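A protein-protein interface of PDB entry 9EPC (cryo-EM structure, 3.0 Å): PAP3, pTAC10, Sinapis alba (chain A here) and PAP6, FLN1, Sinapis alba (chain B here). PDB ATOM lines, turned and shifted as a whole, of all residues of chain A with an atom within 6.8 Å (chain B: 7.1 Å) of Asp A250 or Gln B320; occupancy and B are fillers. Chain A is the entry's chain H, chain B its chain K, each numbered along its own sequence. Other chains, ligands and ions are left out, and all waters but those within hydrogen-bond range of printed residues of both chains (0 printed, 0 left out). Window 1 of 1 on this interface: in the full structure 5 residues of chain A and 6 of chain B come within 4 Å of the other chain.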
ATOM      1  N   SER A 244      21.270   4.210   7.587  1.00  0.00           N
ATOM      2  CA  SER A 244      21.987   4.113   8.853  1.00  0.00           C
ATOM      3  C   SER A 244      21.236   3.235   9.844  1.00  0.00           C
ATOM      4  O   SER A 244      21.837   2.388  10.514  1.00  0.00           O
ATOM      5  CB  SER A 244      22.210   5.506   9.438  1.00  0.00           C
ATOM      6  OG  SER A 244      22.811   5.426  10.717  1.00  0.00           O
ATOM      7  N   TYR A 247      21.405  -0.524   8.639  1.00  0.00           N
ATOM      8  CA  TYR A 247      22.686  -1.214   8.734  1.00  0.00           C
ATOM      9  C   TYR A 247      23.349  -1.096  10.094  1.00  0.00           C
ATOM     10  O   TYR A 247      23.874  -2.088  10.602  1.00  0.00           O
ATOM     11  CB  TYR A 247      23.640  -0.686   7.659  1.00  0.00           C
ATOM     12  CG  TYR A 247      23.131  -0.904   6.255  1.00  0.00           C
ATOM     13  CD1 TYR A 247      22.376  -2.023   5.938  1.00  0.00           C
ATOM     14  CD2 TYR A 247      23.396   0.013   5.250  1.00  0.00           C
ATOM     15  CE1 TYR A 247      21.906  -2.227   4.659  1.00  0.00           C
ATOM     16  CE2 TYR A 247      22.928  -0.182   3.966  1.00  0.00           C
ATOM     17  CZ  TYR A 247      22.184  -1.304   3.677  1.00  0.00           C
ATOM     18  OH  TYR A 247      21.714  -1.505   2.399  1.00  0.00           O
ATOM     19  N   ASP A 248      23.344   0.084  10.706  1.00  0.00           N
ATOM     20  CA  ASP A 248      23.990   0.301  11.994  1.00  0.00           C
ATOM     21  C   ASP A 248      22.935   0.219  13.090  1.00  0.00           C
ATOM     22  O   ASP A 248      22.077   1.100  13.204  1.00  0.00           O
ATOM     23  CB  ASP A 248      24.707   1.647  12.019  1.00  0.00           C
ATOM     24  CG  ASP A 248      25.751   1.767  10.929  1.00  0.00           C
ATOM     25  OD1 ASP A 248      25.904   0.809  10.144  1.00  0.00           O
ATOM     26  OD2 ASP A 248      26.420   2.820  10.858  1.00  0.00           O
ATOM     27  N   GLN A 249      23.002  -0.841  13.897  1.00  0.00           N
ATOM     28  CA  GLN A 249      22.028  -1.023  14.968  1.00  0.00           C
ATOM     29  C   GLN A 249      22.165   0.059  16.030  1.00  0.00           C
ATOM     30  O   GLN A 249      21.178   0.697  16.412  1.00  0.00           O
ATOM     31  CB  GLN A 249      22.190  -2.408  15.590  1.00  0.00           C
ATOM     32  CG  GLN A 249      21.530  -2.550  16.947  1.00  0.00           C
ATOM     33  CD  GLN A 249      21.775  -3.906  17.569  1.00  0.00           C
ATOM     34  OE1 GLN A 249      21.814  -4.922  16.876  1.00  0.00           O
ATOM     35  NE2 GLN A 249      21.952  -3.931  18.882  1.00  0.00           N
ATOM     36  N   ASP A 250      23.381   0.282  16.515  1.00  0.00           N
ATOM     37  CA  ASP A 250      23.643   1.247  17.572  1.00  0.00           C
ATOM     38  C   ASP A 250      24.547   2.352  17.052  1.00  0.00           C
ATOM     39  O   ASP A 250      25.473   2.097  16.278  1.00  0.00           O
ATOM     40  CB  ASP A 250      24.297   0.577  18.781  1.00  0.00           C
ATOM     41  CG  ASP A 250      23.364  -0.373  19.495  1.00  0.00           C
ATOM     42  OD1 ASP A 250      22.145  -0.109  19.514  1.00  0.00           O
ATOM     43  OD2 ASP A 250      23.851  -1.385  20.040  1.00  0.00           O
ATOM     44  N   PHE A 251      24.271   3.580  17.476  1.00  0.00           N
ATOM     45  CA  PHE A 251      25.137   4.689  17.116  1.00  0.00           C
ATOM     46  C   PHE A 251      26.484   4.554  17.809  1.00  0.00           C
ATOM     47  O   PHE A 251      26.563   4.217  18.994  1.00  0.00           O
ATOM     48  CB  PHE A 251      24.499   6.022  17.489  1.00  0.00           C
ATOM     49  CG  PHE A 251      25.431   7.187  17.350  1.00  0.00           C
ATOM     50  CD1 PHE A 251      25.697   7.727  16.107  1.00  0.00           C
ATOM     51  CD2 PHE A 251      26.048   7.734  18.461  1.00  0.00           C
ATOM     52  CE1 PHE A 251      26.558   8.794  15.973  1.00  0.00           C
ATOM     53  CE2 PHE A 251      26.909   8.801  18.332  1.00  0.00           C
ATOM     54  CZ  PHE A 251      27.164   9.333  17.087  1.00  0.00           C
ATOM     55  N   TYR A 252      27.544   4.823  17.061  1.00  0.00           N
ATOM     56  CA  TYR A 252      28.903   4.795  17.566  1.00  0.00           C
ATOM     57  C   TYR A 252      29.658   5.955  16.942  1.00  0.00           C
ATOM     58  O   TYR A 252      29.337   6.370  15.821  1.00  0.00           O
ATOM     59  CB  TYR A 252      29.595   3.468  17.223  1.00  0.00           C
ATOM     60  CG  TYR A 252      30.859   3.205  17.996  1.00  0.00           C
ATOM     61  CD1 TYR A 252      30.812   2.788  19.316  1.00  0.00           C
ATOM     62  CD2 TYR A 252      32.101   3.365  17.404  1.00  0.00           C
ATOM     63  CE1 TYR A 252      31.962   2.546  20.027  1.00  0.00           C
ATOM     64  CE2 TYR A 252      33.257   3.123  18.107  1.00  0.00           C
ATOM     65  CZ  TYR A 252      33.181   2.714  19.416  1.00  0.00           C
ATOM     66  OH  TYR A 252      34.334   2.472  20.118  1.00  0.00           O
ATOM     67  N   ARG A 255      29.880   6.848  13.078  1.00  0.00           N
ATOM     68  CA  ARG A 255      28.686   6.513  12.323  1.00  0.00           C
ATOM     69  C   ARG A 255      27.852   7.765  12.078  1.00  0.00           C
ATOM     70  O   ARG A 255      28.073   8.819  12.676  1.00  0.00           O
ATOM     71  CB  ARG A 255      27.857   5.454  13.051  1.00  0.00           C
ATOM     72  CG  ARG A 255      28.625   4.203  13.437  1.00  0.00           C
ATOM     73  CD  ARG A 255      29.528   3.726  12.316  1.00  0.00           C
ATOM     74  NE  ARG A 255      28.790   3.398  11.105  1.00  0.00           N
ATOM     75  CZ  ARG A 255      29.354   3.178   9.927  1.00  0.00           C
ATOM     76  NH1 ARG A 255      30.663   3.259   9.764  1.00  0.00           N
ATOM     77  NH2 ARG A 255      28.587   2.871   8.887  1.00  0.00           N
ATOM     78  N   ARG A 258      22.111  10.293  13.721  1.00  0.00           N
ATOM     79  CA  ARG A 258      20.724  10.070  13.353  1.00  0.00           C
ATOM     80  C   ARG A 258      19.828  10.433  14.529  1.00  0.00           C
ATOM     81  O   ARG A 258      20.299  10.816  15.603  1.00  0.00           O
ATOM     82  CB  ARG A 258      20.506   8.614  12.926  1.00  0.00           C
ATOM     83  CG  ARG A 258      20.904   7.615  13.991  1.00  0.00           C
ATOM     84  CD  ARG A 258      21.075   6.226  13.418  1.00  0.00           C
ATOM     85  NE  ARG A 258      21.374   5.252  14.458  1.00  0.00           N
ATOM     86  CZ  ARG A 258      21.659   3.977  14.231  1.00  0.00           C
ATOM     87  NH1 ARG A 258      21.715   3.491  13.002  1.00  0.00           N
ATOM     88  NH2 ARG A 258      21.897   3.172  15.262  1.00  0.00           N
ATOM     89  N   PHE A 363      33.876  -3.126   8.859  1.00  0.00           N
ATOM     90  CA  PHE A 363      32.746  -3.913   9.315  1.00  0.00           C
ATOM     91  C   PHE A 363      32.774  -5.304   8.693  1.00  0.00           C
ATOM     92  O   PHE A 363      33.540  -5.593   7.772  1.00  0.00           O
ATOM     93  CB  PHE A 363      31.431  -3.225   8.962  1.00  0.00           C
ATOM     94  CG  PHE A 363      31.019  -2.166   9.932  1.00  0.00           C
ATOM     95  CD1 PHE A 363      30.513  -2.509  11.170  1.00  0.00           C
ATOM     96  CD2 PHE A 363      31.112  -0.832   9.600  1.00  0.00           C
ATOM     97  CE1 PHE A 363      30.122  -1.540  12.062  1.00  0.00           C
ATOM     98  CE2 PHE A 363      30.718   0.140  10.489  1.00  0.00           C
ATOM     99  CZ  PHE A 363      30.226  -0.214  11.722  1.00  0.00           C
ATOM    100  N   ARG A 365      29.488  -7.075   7.510  1.00  0.00           N
ATOM    101  CA  ARG A 365      28.047  -6.911   7.440  1.00  0.00           C
ATOM    102  C   ARG A 365      27.357  -8.266   7.308  1.00  0.00           C
ATOM    103  O   ARG A 365      27.980  -9.329   7.374  1.00  0.00           O
ATOM    104  CB  ARG A 365      27.683  -5.995   6.276  1.00  0.00           C
ATOM    105  CG  ARG A 365      28.241  -4.594   6.405  1.00  0.00           C
ATOM    106  CD  ARG A 365      27.601  -3.860   7.563  1.00  0.00           C
ATOM    107  NE  ARG A 365      28.053  -2.478   7.645  1.00  0.00           N
ATOM    108  CZ  ARG A 365      27.565  -1.580   8.488  1.00  0.00           C
ATOM    109  NH1 ARG A 365      26.595  -1.883   9.334  1.00  0.00           N
ATOM    110  NH2 ARG A 365      28.060  -0.347   8.480  1.00  0.00           N
ATOM    111  N   TYR B 317      17.235  -8.222  21.719  1.00  0.00           N
ATOM    112  CA  TYR B 317      18.117  -7.090  21.479  1.00  0.00           C
ATOM    113  C   TYR B 317      19.365  -7.195  22.344  1.00  0.00           C
ATOM    114  O   TYR B 317      19.279  -7.388  23.560  1.00  0.00           O
ATOM    115  CB  TYR B 317      17.389  -5.780  21.767  1.00  0.00           C
ATOM    116  CG  TYR B 317      18.284  -4.565  21.716  1.00  0.00           C
ATOM    117  CD1 TYR B 317      18.543  -3.922  20.517  1.00  0.00           C
ATOM    118  CD2 TYR B 317      18.869  -4.060  22.869  1.00  0.00           C
ATOM    119  CE1 TYR B 317      19.359  -2.813  20.464  1.00  0.00           C
ATOM    120  CE2 TYR B 317      19.688  -2.955  22.826  1.00  0.00           C
ATOM    121  CZ  TYR B 317      19.930  -2.334  21.623  1.00  0.00           C
ATOM    122  OH  TYR B 317      20.745  -1.228  21.577  1.00  0.00           O
ATOM    123  N   THR B 318      20.528  -7.058  21.711  1.00  0.00           N
ATOM    124  CA  THR B 318      21.801  -6.986  22.408  1.00  0.00           C
ATOM    125  C   THR B 318      22.543  -5.761  21.892  1.00  0.00           C
ATOM    126  O   THR B 318      22.630  -5.564  20.667  1.00  0.00           O
ATOM    127  CB  THR B 318      22.645  -8.248  22.193  1.00  0.00           C
ATOM    128  OG1 THR B 318      22.913  -8.412  20.796  1.00  0.00           O
ATOM    129  CG2 THR B 318      21.918  -9.474  22.714  1.00  0.00           C
ATOM    130  N   PRO B 319      23.071  -4.914  22.771  1.00  0.00           N
ATOM    131  CA  PRO B 319      23.805  -3.733  22.303  1.00  0.00           C
ATOM    132  C   PRO B 319      25.004  -4.134  21.460  1.00  0.00           C
ATOM    133  O   PRO B 319      25.693  -5.113  21.749  1.00  0.00           O
ATOM    134  CB  PRO B 319      24.224  -3.033  23.600  1.00  0.00           C
ATOM    135  CG  PRO B 319      24.102  -4.066  24.659  1.00  0.00           C
ATOM    136  CD  PRO B 319      23.007  -4.982  24.238  1.00  0.00           C
ATOM    137  N   GLN B 320      25.246  -3.359  20.404  1.00  0.00           N
ATOM    138  CA  GLN B 320      26.224  -3.761  19.400  1.00  0.00           C
ATOM    139  C   GLN B 320      27.652  -3.592  19.902  1.00  0.00           C
ATOM    140  O   GLN B 320      28.506  -4.450  19.652  1.00  0.00           O
ATOM    141  CB  GLN B 320      26.007  -2.959  18.118  1.00  0.00           C
ATOM    142  CG  GLN B 320      26.890  -3.382  16.965  1.00  0.00           C
ATOM    143  CD  GLN B 320      26.658  -2.544  15.729  1.00  0.00           C
ATOM    144  OE1 GLN B 320      25.875  -1.596  15.747  1.00  0.00           O
ATOM    145  NE2 GLN B 320      27.338  -2.889  14.645  1.00  0.00           N
ATOM    146  N   TYR B 321      27.933  -2.503  20.610  1.00  0.00           N
ATOM    147  CA  TYR B 321      29.299  -2.165  20.992  1.00  0.00           C
ATOM    148  C   TYR B 321      29.592  -2.354  22.469  1.00  0.00           C
ATOM    149  O   TYR B 321      30.635  -2.910  22.815  1.00  0.00           O
ATOM    150  CB  TYR B 321      29.606  -0.719  20.598  1.00  0.00           C
ATOM    151  CG  TYR B 321      29.473  -0.470  19.118  1.00  0.00           C
ATOM    152  CD1 TYR B 321      30.515  -0.759  18.251  1.00  0.00           C
ATOM    153  CD2 TYR B 321      28.305   0.048  18.586  1.00  0.00           C
ATOM    154  CE1 TYR B 321      30.397  -0.536  16.897  1.00  0.00           C
ATOM    155  CE2 TYR B 321      28.177   0.273  17.234  1.00  0.00           C
ATOM    156  CZ  TYR B 321      29.226  -0.019  16.395  1.00  0.00           C
ATOM    157  OH  TYR B 321      29.102   0.206  15.046  1.00  0.00           O
ATOM    158  N   PHE B 322      28.712  -1.902  23.356  1.00  0.00           N
ATOM    159  CA  PHE B 322      28.940  -2.071  24.783  1.00  0.00           C
ATOM    160  C   PHE B 322      27.609  -1.995  25.511  1.00  0.00           C
ATOM    161  O   PHE B 322      26.644  -1.403  25.022  1.00  0.00           O
ATOM    162  CB  PHE B 322      29.914  -1.019  25.324  1.00  0.00           C
ATOM    163  CG  PHE B 322      29.597   0.379  24.890  1.00  0.00           C
ATOM    164  CD1 PHE B 322      28.680   1.144  25.584  1.00  0.00           C
ATOM    165  CD2 PHE B 322      30.218   0.928  23.784  1.00  0.00           C
ATOM    166  CE1 PHE B 322      28.387   2.426  25.183  1.00  0.00           C
ATOM    167  CE2 PHE B 322      29.929   2.211  23.379  1.00  0.00           C
ATOM    168  CZ  PHE B 322      29.012   2.961  24.080  1.00  0.00           C
ATOM    169  N   ALA B 323      27.573  -2.604  26.691  1.00  0.00           N
ATOM    170  CA  ALA B 323      26.380  -2.572  27.519  1.00  0.00           C
ATOM    171  C   ALA B 323      26.160  -1.181  28.098  1.00  0.00           C
ATOM    172  O   ALA B 323      27.108  -0.440  28.367  1.00  0.00           O
ATOM    173  CB  ALA B 323      26.489  -3.592  28.648  1.00  0.00           C
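OH of Tyr B317 lies within hydrogen-bond range of OD1 of Asp A250, 2.7 Å away.
O of Thr B318 is in hydrogen-bond range of NE2 of Gln A249.
OE1 of Gln B320 lies within hydrogen-bond range of N of Gln A249 (3.5 Å).
The side-chain carboxylate (OD2) of Asp A250 lies within hydrogen-bond range of the backbone NH (N) of Gln B320.
Along chain B the printed residues that touch a printed residue of chain A span positions 317 to 322.
Among the printed residues, no Asp or Glu carboxylate lies within 4 Å of a Lys or Arg side-chain nitrogen of the other chain.
OD2 of Asp A250 lies within hydrogen-bond range of NE2 of Gln A249, 3.4 Å away.
The backbone carbonyl oxygen of Gln A249 lies within hydrogen-bond range of the guanidinium group of Arg A258 (2.8 Å).
Of chain B, only Tyr B317 (2.7 Å), Pro B319 (3.3 Å), Gln B320 (2.4 Å) and Tyr B321 (3.4 Å) come within 4 Å of Asp A250.
Printed residues of chain A within 4 Å of Gln B320: Gln A249 and Asp A250.
Printed residues of chain A within 4 Å of Phe B322: Tyr A252 (3.9 Å).
Of the printed residues of chain B, Gln A249 touches Tyr B317 (3.2 Å), Thr B318 (2.5 Å), Pro B319 (3.9 Å) and Gln B320 (3.5 Å).
Of the printed residues of chain B, Tyr A252 touches Tyr B321 (3.5 Å) and Phe B322 (3.9 Å).
Of the printed residues of chain A, Tyr B317 touches Gln A249 and Asp A250.
Of the printed residues of chain A, Thr B318 touches Gln A249.
Tyr A247 touches none of the printed residues of chain B.
Ala B323 touches none of the printed residues of chain A.
Among the printed residues, merely in contact across the chains: Gln A249 with Tyr B317, Gln A249 with Pro B319, Asp A250 with Pro B319, Asp A250 with Tyr B321, Tyr A252 with Tyr B321, Tyr A252 with Phe B322 and Phe A363 with Tyr B321.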
